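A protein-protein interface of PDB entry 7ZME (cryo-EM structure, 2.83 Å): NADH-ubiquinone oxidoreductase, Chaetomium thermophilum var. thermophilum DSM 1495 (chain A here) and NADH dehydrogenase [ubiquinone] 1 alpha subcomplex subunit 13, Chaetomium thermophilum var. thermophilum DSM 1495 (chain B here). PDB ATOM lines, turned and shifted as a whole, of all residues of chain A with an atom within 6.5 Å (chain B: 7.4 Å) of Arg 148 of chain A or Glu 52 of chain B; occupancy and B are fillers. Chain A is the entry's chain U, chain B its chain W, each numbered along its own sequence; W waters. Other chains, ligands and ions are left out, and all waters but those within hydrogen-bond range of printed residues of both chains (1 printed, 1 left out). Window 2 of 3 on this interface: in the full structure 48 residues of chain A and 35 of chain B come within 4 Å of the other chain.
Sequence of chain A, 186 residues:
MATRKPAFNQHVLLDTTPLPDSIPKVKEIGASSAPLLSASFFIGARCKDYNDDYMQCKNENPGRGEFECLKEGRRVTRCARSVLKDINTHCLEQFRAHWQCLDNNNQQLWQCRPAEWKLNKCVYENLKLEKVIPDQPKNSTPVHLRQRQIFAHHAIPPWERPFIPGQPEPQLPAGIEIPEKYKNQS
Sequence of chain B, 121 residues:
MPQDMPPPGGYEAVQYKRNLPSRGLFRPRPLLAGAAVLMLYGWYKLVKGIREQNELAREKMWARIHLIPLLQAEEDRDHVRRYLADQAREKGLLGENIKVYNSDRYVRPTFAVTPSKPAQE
NH2 of Arg 146 of chain A is in salt-bridge range of OE1 of Glu 52 of chain B. The side-chain carboxylate (OE2) of Glu 52 of chain B lies within hydrogen-bond range of the side-chain amide nitrogen (NE2) of Gln 149 of chain A, at 3.5 Å.
Of the 11 printed residues of chain A, 6 touch a printed residue of chain B. Printed residues of chain A that touch a printed residue of chain B: Val 143, Arg 146, Arg 148, Gln 149, Ile 150 and Phe 151. Along chain A the printed residues that touch a printed residue of chain B span positions 143 to 151. Of the 13 printed residues of chain B, 5 touch a printed residue of chain A. Along chain B the printed residues that touch a printed residue of chain A span positions 49 to 56. Among the printed residues, 10 pairs touch across the chains. Among the printed residues, Asp or Glu carboxylates within 4 Å of a Lys or Arg side-chain nitrogen of the other chain: Arg 146 of chain A with Glu 52 of chain B (2.9 Å).
Glu 52 of chain B touches Val 143 of chain A. Val 143 of chain A touches Glu 55 of chain B (CG1 to O, 3.9 Å). CD2 of Leu 56 of chain B touches CG2 of Val 143 of chain A, 3.6 Å away. O of Arg 148 of chain A touches OE2 of Glu 52 of chain B, 3.8 Å away. Ile 150 of chain A touches Glu 52 of chain B (N to OE2, 3.5 Å). Phe 151 of chain A touches Gly 49 of chain B. Phe 151 of chain A touches Gln 53 of chain B (CE2 to CB, 3.8 Å). Phe 151 of chain A touches Leu 56 of chain B.
The backbone carbonyl oxygen (O) of Val 143 of chain A lies close to the side-chain amide oxygen (OE1) of Gln 149 of chain A (2.9 Å). The backbone carbonyl oxygen of Arg 146 of chain A sits close to the side-chain amide oxygen of Gln 149 of chain A (3.1 Å). OE2 of Glu 55 of chain B lies within salt-bridge range of NE of Arg 58 of chain B (2.8 Å).
Water W1 lies within hydrogen-bond range of the guanidinium group (NH2) of Arg 146 of chain A (3.3 Å), the backbone carbonyl oxygen (O) of Lys 48 of chain B (3.3 Å) and the backbone NH (N) of Glu 52 of chain B (3.5 Å).
Of chain B, only Glu 52 comes within 4 Å of Arg 148 of chain A. Of the printed residues of chain B, Ile 150 of chain A touches Glu 52. Printed residues of chain A within 4 Å of Gln 53 of chain B: Phe 151. Of the printed residues of chain A, Leu 56 of chain B touches Val 143 and Phe 151. The nearest residue of chain A that does not touch Glu 52 of chain B is Phe 151 of chain A (4.4 Å).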
ATOM      1  N   TRP A 117       9.539   5.581  -6.182  1.00  0.00           N
ATOM      2  CA  TRP A 117      10.327   4.643  -7.019  1.00  0.00           C
ATOM      3  C   TRP A 117      11.697   5.258  -7.281  1.00  0.00           C
ATOM      4  O   TRP A 117      12.697   4.521  -7.231  1.00  0.00           O
ATOM      5  CB  TRP A 117       9.603   4.275  -8.317  1.00  0.00           C
ATOM      6  CG  TRP A 117       8.315   3.542  -8.102  1.00  0.00           C
ATOM      7  CD1 TRP A 117       8.010   2.708  -7.068  1.00  0.00           C
ATOM      8  CD2 TRP A 117       7.148   3.579  -8.944  1.00  0.00           C
ATOM      9  NE1 TRP A 117       6.737   2.227  -7.204  1.00  0.00           N
ATOM     10  CE2 TRP A 117       6.185   2.740  -8.347  1.00  0.00           C
ATOM     11  CE3 TRP A 117       6.825   4.230 -10.137  1.00  0.00           C
ATOM     12  CZ2 TRP A 117       4.925   2.534  -8.907  1.00  0.00           C
ATOM     13  CZ3 TRP A 117       5.580   4.029 -10.689  1.00  0.00           C
ATOM     14  CH2 TRP A 117       4.645   3.193 -10.081  1.00  0.00           C
ATOM     15  N   VAL A 143       1.442  -4.099  -3.903  1.00  0.00           N
ATOM     16  CA  VAL A 143       0.701  -2.838  -4.214  1.00  0.00           C
ATOM     17  C   VAL A 143       1.657  -1.660  -4.459  1.00  0.00           C
ATOM     18  O   VAL A 143       1.304  -0.781  -5.255  1.00  0.00           O
ATOM     19  CB  VAL A 143      -0.393  -2.532  -3.168  1.00  0.00           C
ATOM     20  CG1 VAL A 143       0.185  -1.963  -1.881  1.00  0.00           C
ATOM     21  CG2 VAL A 143      -1.481  -1.632  -3.727  1.00  0.00           C
ATOM     22  N   ARG A 146       3.132  -1.589  -8.089  1.00  0.00           N
ATOM     23  CA  ARG A 146       2.057  -1.692  -9.110  1.00  0.00           C
ATOM     24  C   ARG A 146       2.058  -0.433  -9.972  1.00  0.00           C
ATOM     25  O   ARG A 146       2.130   0.657  -9.400  1.00  0.00           O
ATOM     26  CB  ARG A 146       0.690  -1.889  -8.451  1.00  0.00           C
ATOM     27  CG  ARG A 146       0.317  -3.332  -8.169  1.00  0.00           C
ATOM     28  CD  ARG A 146      -1.009  -3.469  -7.452  1.00  0.00           C
ATOM     29  NE  ARG A 146      -1.142  -4.818  -6.926  1.00  0.00           N
ATOM     30  CZ  ARG A 146      -2.075  -5.206  -6.072  1.00  0.00           C
ATOM     31  NH1 ARG A 146      -2.103  -6.459  -5.654  1.00  0.00           N
ATOM     32  NH2 ARG A 146      -2.972  -4.343  -5.630  1.00  0.00           N
ATOM     33  N   GLN A 147       1.984  -0.586 -11.291  1.00  0.00           N
ATOM     34  CA  GLN A 147       2.013   0.560 -12.233  1.00  0.00           C
ATOM     35  C   GLN A 147       0.797   1.446 -12.008  1.00  0.00           C
ATOM     36  O   GLN A 147       0.966   2.669 -11.933  1.00  0.00           O
ATOM     37  CB  GLN A 147       2.020   0.040 -13.668  1.00  0.00           C
ATOM     38  CG  GLN A 147       2.086   1.143 -14.715  1.00  0.00           C
ATOM     39  CD  GLN A 147       3.402   1.879 -14.687  1.00  0.00           C
ATOM     40  OE1 GLN A 147       4.458   1.293 -14.464  1.00  0.00           O
ATOM     41  NE2 GLN A 147       3.348   3.177 -14.932  1.00  0.00           N
ATOM     42  N   ARG A 148      -0.381   0.845 -11.890  1.00  0.00           N
ATOM     43  CA  ARG A 148      -1.618   1.639 -11.794  1.00  0.00           C
ATOM     44  C   ARG A 148      -2.074   1.686 -10.341  1.00  0.00           C
ATOM     45  O   ARG A 148      -2.127   0.618  -9.697  1.00  0.00           O
ATOM     46  CB  ARG A 148      -2.686   0.969 -12.649  1.00  0.00           C
ATOM     47  CG  ARG A 148      -2.342   0.904 -14.130  1.00  0.00           C
ATOM     48  CD  ARG A 148      -3.572   0.661 -14.983  1.00  0.00           C
ATOM     49  NE  ARG A 148      -4.606   1.654 -14.726  1.00  0.00           N
ATOM     50  CZ  ARG A 148      -4.727   2.806 -15.375  1.00  0.00           C
ATOM     51  NH1 ARG A 148      -5.703   3.640 -15.065  1.00  0.00           N
ATOM     52  NH2 ARG A 148      -3.873   3.119 -16.333  1.00  0.00           N
ATOM     53  N   GLN A 149      -2.363   2.879  -9.836  1.00  0.00           N
ATOM     54  CA  GLN A 149      -2.922   2.967  -8.476  1.00  0.00           C
ATOM     55  C   GLN A 149      -4.409   3.301  -8.615  1.00  0.00           C
ATOM     56  O   GLN A 149      -4.712   4.318  -9.224  1.00  0.00           O
ATOM     57  CB  GLN A 149      -2.090   3.935  -7.641  1.00  0.00           C
ATOM     58  CG  GLN A 149      -0.645   3.498  -7.448  1.00  0.00           C
ATOM     59  CD  GLN A 149      -0.456   2.227  -6.655  1.00  0.00           C
ATOM     60  OE1 GLN A 149       0.513   1.499  -6.850  1.00  0.00           O
ATOM     61  NE2 GLN A 149      -1.364   1.954  -5.735  1.00  0.00           N
ATOM     62  N   ILE A 150      -5.296   2.512  -8.013  1.00  0.00           N
ATOM     63  CA  ILE A 150      -6.751   2.744  -8.239  1.00  0.00           C
ATOM     64  C   ILE A 150      -7.222   3.907  -7.361  1.00  0.00           C
ATOM     65  O   ILE A 150      -8.195   4.574  -7.753  1.00  0.00           O
ATOM     66  CB  ILE A 150      -7.521   1.462  -7.854  1.00  0.00           C
ATOM     67  CG1 ILE A 150      -7.014   0.228  -8.603  1.00  0.00           C
ATOM     68  CG2 ILE A 150      -9.024   1.635  -8.012  1.00  0.00           C
ATOM     69  CD1 ILE A 150      -7.770  -1.032  -8.267  1.00  0.00           C
ATOM     70  N   PHE A 151      -6.519   4.197  -6.266  1.00  0.00           N
ATOM     71  CA  PHE A 151      -6.999   5.241  -5.327  1.00  0.00           C
ATOM     72  C   PHE A 151      -6.182   6.518  -5.498  1.00  0.00           C
ATOM     73  O   PHE A 151      -6.457   7.496  -4.783  1.00  0.00           O
ATOM     74  CB  PHE A 151      -7.111   4.680  -3.909  1.00  0.00           C
ATOM     75  CG  PHE A 151      -8.111   3.562  -3.783  1.00  0.00           C
ATOM     76  CD1 PHE A 151      -9.463   3.833  -3.649  1.00  0.00           C
ATOM     77  CD2 PHE A 151      -7.705   2.239  -3.829  1.00  0.00           C
ATOM     78  CE1 PHE A 151     -10.387   2.807  -3.545  1.00  0.00           C
ATOM     79  CE2 PHE A 151      -8.631   1.215  -3.728  1.00  0.00           C
ATOM     80  CZ  PHE A 151      -9.968   1.499  -3.584  1.00  0.00           C
ATOM     81  N   ALA A 152      -5.242   6.517  -6.446  1.00  0.00           N
ATOM     82  CA  ALA A 152      -4.413   7.718  -6.713  1.00  0.00           C
ATOM     83  C   ALA A 152      -5.219   8.729  -7.519  1.00  0.00           C
ATOM     84  O   ALA A 152      -5.742   8.337  -8.569  1.00  0.00           O
ATOM     85  CB  ALA A 152      -3.152   7.346  -7.436  1.00  0.00           C
ATOM     86  N   ALA A 155      -3.327   9.682 -12.375  1.00  0.00           N
ATOM     87  CA  ALA A 155      -2.851   8.390 -12.916  1.00  0.00           C
ATOM     88  C   ALA A 155      -1.333   8.409 -13.051  1.00  0.00           C
ATOM     89  O   ALA A 155      -0.777   9.490 -13.269  1.00  0.00           O
ATOM     90  CB  ALA A 155      -3.530   8.095 -14.226  1.00  0.00           C
ATOM     91  N   ILE A 156      -0.693   7.249 -12.904  1.00  0.00           N
ATOM     92  CA  ILE A 156       0.795   7.194 -12.928  1.00  0.00           C
ATOM     93  C   ILE A 156       1.197   7.203 -14.389  1.00  0.00           C
ATOM     94  O   ILE A 156       0.659   6.394 -15.143  1.00  0.00           O
ATOM     95  CB  ILE A 156       1.360   5.980 -12.148  1.00  0.00           C
ATOM     96  CG1 ILE A 156       1.252   6.169 -10.633  1.00  0.00           C
ATOM     97  CG2 ILE A 156       2.796   5.696 -12.551  1.00  0.00           C
ATOM     98  CD1 ILE A 156      -0.139   6.018 -10.084  1.00  0.00           C
ATOM     99  N   LEU B  46     -15.409  -3.957  -7.522  1.00  0.00           N
ATOM    100  CA  LEU B  46     -15.373  -3.791  -6.076  1.00  0.00           C
ATOM    101  C   LEU B  46     -14.457  -4.818  -5.424  1.00  0.00           C
ATOM    102  O   LEU B  46     -13.793  -4.517  -4.428  1.00  0.00           O
ATOM    103  CB  LEU B  46     -16.787  -3.886  -5.509  1.00  0.00           C
ATOM    104  CG  LEU B  46     -16.971  -3.331  -4.099  1.00  0.00           C
ATOM    105  CD1 LEU B  46     -17.198  -1.827  -4.129  1.00  0.00           C
ATOM    106  CD2 LEU B  46     -18.109  -4.040  -3.400  1.00  0.00           C
ATOM    107  N   VAL B  47     -14.437  -6.048  -5.940  1.00  0.00           N
ATOM    108  CA  VAL B  47     -13.487  -7.068  -5.412  1.00  0.00           C
ATOM    109  C   VAL B  47     -12.069  -6.508  -5.535  1.00  0.00           C
ATOM    110  O   VAL B  47     -11.390  -6.422  -4.511  1.00  0.00           O
ATOM    111  CB  VAL B  47     -13.653  -8.460  -6.057  1.00  0.00           C
ATOM    112  CG1 VAL B  47     -12.442  -9.346  -5.829  1.00  0.00           C
ATOM    113  CG2 VAL B  47     -14.917  -9.156  -5.581  1.00  0.00           C
ATOM    114  N   LYS B  48     -11.684  -6.070  -6.734  1.00  0.00           N
ATOM    115  CA  LYS B  48     -10.320  -5.553  -6.997  1.00  0.00           C
ATOM    116  C   LYS B  48     -10.020  -4.327  -6.142  1.00  0.00           C
ATOM    117  O   LYS B  48      -8.903  -4.258  -5.619  1.00  0.00           O
ATOM    118  CB  LYS B  48     -10.247  -5.141  -8.470  1.00  0.00           C
ATOM    119  CG  LYS B  48     -10.504  -6.249  -9.482  1.00  0.00           C
ATOM    120  CD  LYS B  48      -9.356  -7.224  -9.584  1.00  0.00           C
ATOM    121  CE  LYS B  48      -8.045  -6.542  -9.914  1.00  0.00           C
ATOM    122  NZ  LYS B  48      -6.889  -7.453  -9.736  1.00  0.00           N
ATOM    123  N   GLY B  49     -10.977  -3.405  -6.002  1.00  0.00           N
ATOM    124  CA  GLY B  49     -10.761  -2.169  -5.232  1.00  0.00           C
ATOM    125  C   GLY B  49     -10.450  -2.432  -3.780  1.00  0.00           C
ATOM    126  O   GLY B  49      -9.484  -1.852  -3.273  1.00  0.00           O
ATOM    127  N   ILE B  50     -11.310  -3.206  -3.119  1.00  0.00           N
ATOM    128  CA  ILE B  50     -11.151  -3.494  -1.665  1.00  0.00           C
ATOM    129  C   ILE B  50      -9.897  -4.335  -1.444  1.00  0.00           C
ATOM    130  O   ILE B  50      -9.206  -4.108  -0.450  1.00  0.00           O
ATOM    131  CB  ILE B  50     -12.425  -4.125  -1.068  1.00  0.00           C
ATOM    132  CG1 ILE B  50     -13.669  -3.297  -1.399  1.00  0.00           C
ATOM    133  CG2 ILE B  50     -12.284  -4.344   0.429  1.00  0.00           C
ATOM    134  CD1 ILE B  50     -14.956  -3.889  -0.885  1.00  0.00           C
ATOM    135  N   ARG B  51      -9.621  -5.268  -2.347  1.00  0.00           N
ATOM    136  CA  ARG B  51      -8.393  -6.081  -2.213  1.00  0.00           C
ATOM    137  C   ARG B  51      -7.178  -5.151  -2.275  1.00  0.00           C
ATOM    138  O   ARG B  51      -6.280  -5.325  -1.440  1.00  0.00           O
ATOM    139  CB  ARG B  51      -8.425  -7.236  -3.215  1.00  0.00           C
ATOM    140  CG  ARG B  51      -9.318  -8.387  -2.777  1.00  0.00           C
ATOM    141  CD  ARG B  51      -9.162  -9.605  -3.656  1.00  0.00           C
ATOM    142  NE  ARG B  51     -10.123 -10.660  -3.377  1.00  0.00           N
ATOM    143  CZ  ARG B  51     -10.241 -11.765  -4.102  1.00  0.00           C
ATOM    144  NH1 ARG B  51     -11.149 -12.673  -3.788  1.00  0.00           N
ATOM    145  NH2 ARG B  51      -9.454 -11.953  -5.144  1.00  0.00           N
ATOM    146  N   GLU B  52      -7.180  -4.172  -3.184  1.00  0.00           N
ATOM    147  CA  GLU B  52      -6.077  -3.180  -3.299  1.00  0.00           C
ATOM    148  C   GLU B  52      -6.001  -2.301  -2.053  1.00  0.00           C
ATOM    149  O   GLU B  52      -4.882  -2.023  -1.617  1.00  0.00           O
ATOM    150  CB  GLU B  52      -6.268  -2.346  -4.565  1.00  0.00           C
ATOM    151  CG  GLU B  52      -5.216  -1.275  -4.768  1.00  0.00           C
ATOM    152  CD  GLU B  52      -4.533  -1.329  -6.121  1.00  0.00           C
ATOM    153  OE1 GLU B  52      -4.671  -2.357  -6.806  1.00  0.00           O
ATOM    154  OE2 GLU B  52      -3.872  -0.342  -6.490  1.00  0.00           O
ATOM    155  N   GLN B  53      -7.148  -1.849  -1.535  1.00  0.00           N
ATOM    156  CA  GLN B  53      -7.184  -0.957  -0.344  1.00  0.00           C
ATOM    157  C   GLN B  53      -6.705  -1.691   0.915  1.00  0.00           C
ATOM    158  O   GLN B  53      -6.031  -1.059   1.725  1.00  0.00           O
ATOM    159  CB  GLN B  53      -8.521  -0.231  -0.210  1.00  0.00           C
ATOM    160  CG  GLN B  53      -9.581  -0.998   0.557  1.00  0.00           C
ATOM    161  CD  GLN B  53     -10.865  -0.218   0.659  1.00  0.00           C
ATOM    162  OE1 GLN B  53     -11.040   0.816   0.018  1.00  0.00           O
ATOM    163  NE2 GLN B  53     -11.777  -0.713   1.476  1.00  0.00           N
ATOM    164  N   ASN B  54      -7.059  -2.962   1.076  1.00  0.00           N
ATOM    165  CA  ASN B  54      -6.619  -3.745   2.252  1.00  0.00           C
ATOM    166  C   ASN B  54      -5.103  -3.884   2.173  1.00  0.00           C
ATOM    167  O   ASN B  54      -4.475  -3.943   3.237  1.00  0.00           O
ATOM    168  CB  ASN B  54      -7.404  -5.052   2.408  1.00  0.00           C
ATOM    169  CG  ASN B  54      -8.848  -4.837   2.805  1.00  0.00           C
ATOM    170  OD1 ASN B  54      -9.279  -3.707   3.018  1.00  0.00           O
ATOM    171  ND2 ASN B  54      -9.604  -5.914   2.911  1.00  0.00           N
ATOM    172  N   GLU B  55      -4.549  -3.949   0.961  1.00  0.00           N
ATOM    173  CA  GLU B  55      -3.075  -3.980   0.771  1.00  0.00           C
ATOM    174  C   GLU B  55      -2.448  -2.608   1.048  1.00  0.00           C
ATOM    175  O   GLU B  55      -1.360  -2.579   1.637  1.00  0.00           O
ATOM    176  CB  GLU B  55      -2.758  -4.586  -0.592  1.00  0.00           C
ATOM    177  CG  GLU B  55      -3.085  -6.062  -0.655  1.00  0.00           C
ATOM    178  CD  GLU B  55      -2.654  -6.821   0.587  1.00  0.00           C
ATOM    179  OE1 GLU B  55      -3.513  -7.475   1.211  1.00  0.00           O
ATOM    180  OE2 GLU B  55      -1.456  -6.764   0.924  1.00  0.00           O
ATOM    181  N   LEU B  56      -3.089  -1.520   0.630  1.00  0.00           N
ATOM    182  CA  LEU B  56      -2.612  -0.144   0.925  1.00  0.00           C
ATOM    183  C   LEU B  56      -2.633   0.062   2.436  1.00  0.00           C
ATOM    184  O   LEU B  56      -1.749   0.769   2.941  1.00  0.00           O
ATOM    185  CB  LEU B  56      -3.558   0.846   0.243  1.00  0.00           C
ATOM    186  CG  LEU B  56      -3.450   0.951  -1.276  1.00  0.00           C
ATOM    187  CD1 LEU B  56      -4.439   1.974  -1.802  1.00  0.00           C
ATOM    188  CD2 LEU B  56      -2.039   1.323  -1.685  1.00  0.00           C
ATOM    189  N   ALA B  57      -3.643  -0.490   3.110  1.00  0.00           N
ATOM    190  CA  ALA B  57      -3.749  -0.411   4.584  1.00  0.00           C
ATOM    191  C   ALA B  57      -2.574  -1.135   5.242  1.00  0.00           C
ATOM    192  O   ALA B  57      -2.103  -0.650   6.275  1.00  0.00           O
ATOM    193  CB  ALA B  57      -5.075  -0.960   5.023  1.00  0.00           C
ATOM    194  N   ARG B  58      -2.136  -2.260   4.672  1.00  0.00           N
ATOM    195  CA  ARG B  58      -0.973  -3.019   5.207  1.00  0.00           C
ATOM    196  C   ARG B  58       0.295  -2.172   5.114  1.00  0.00           C
ATOM    197  O   ARG B  58       1.087  -2.203   6.060  1.00  0.00           O
ATOM    198  CB  ARG B  58      -0.811  -4.326   4.433  1.00  0.00           C
ATOM    199  CG  ARG B  58       0.278  -5.243   4.968  1.00  0.00           C
ATOM    200  CD  ARG B  58       0.532  -6.426   4.055  1.00  0.00           C
ATOM    201  NE  ARG B  58      -0.706  -7.043   3.608  1.00  0.00           N
ATOM    202  CZ  ARG B  58      -1.368  -7.983   4.270  1.00  0.00           C
ATOM    203  NH1 ARG B  58      -2.487  -8.470   3.767  1.00  0.00           N
ATOM    204  NH2 ARG B  58      -0.915  -8.431   5.426  1.00  0.00           N
HETATM  205  O   HOH W   1      -5.911  -5.701  -6.023  1.00  0.00           O
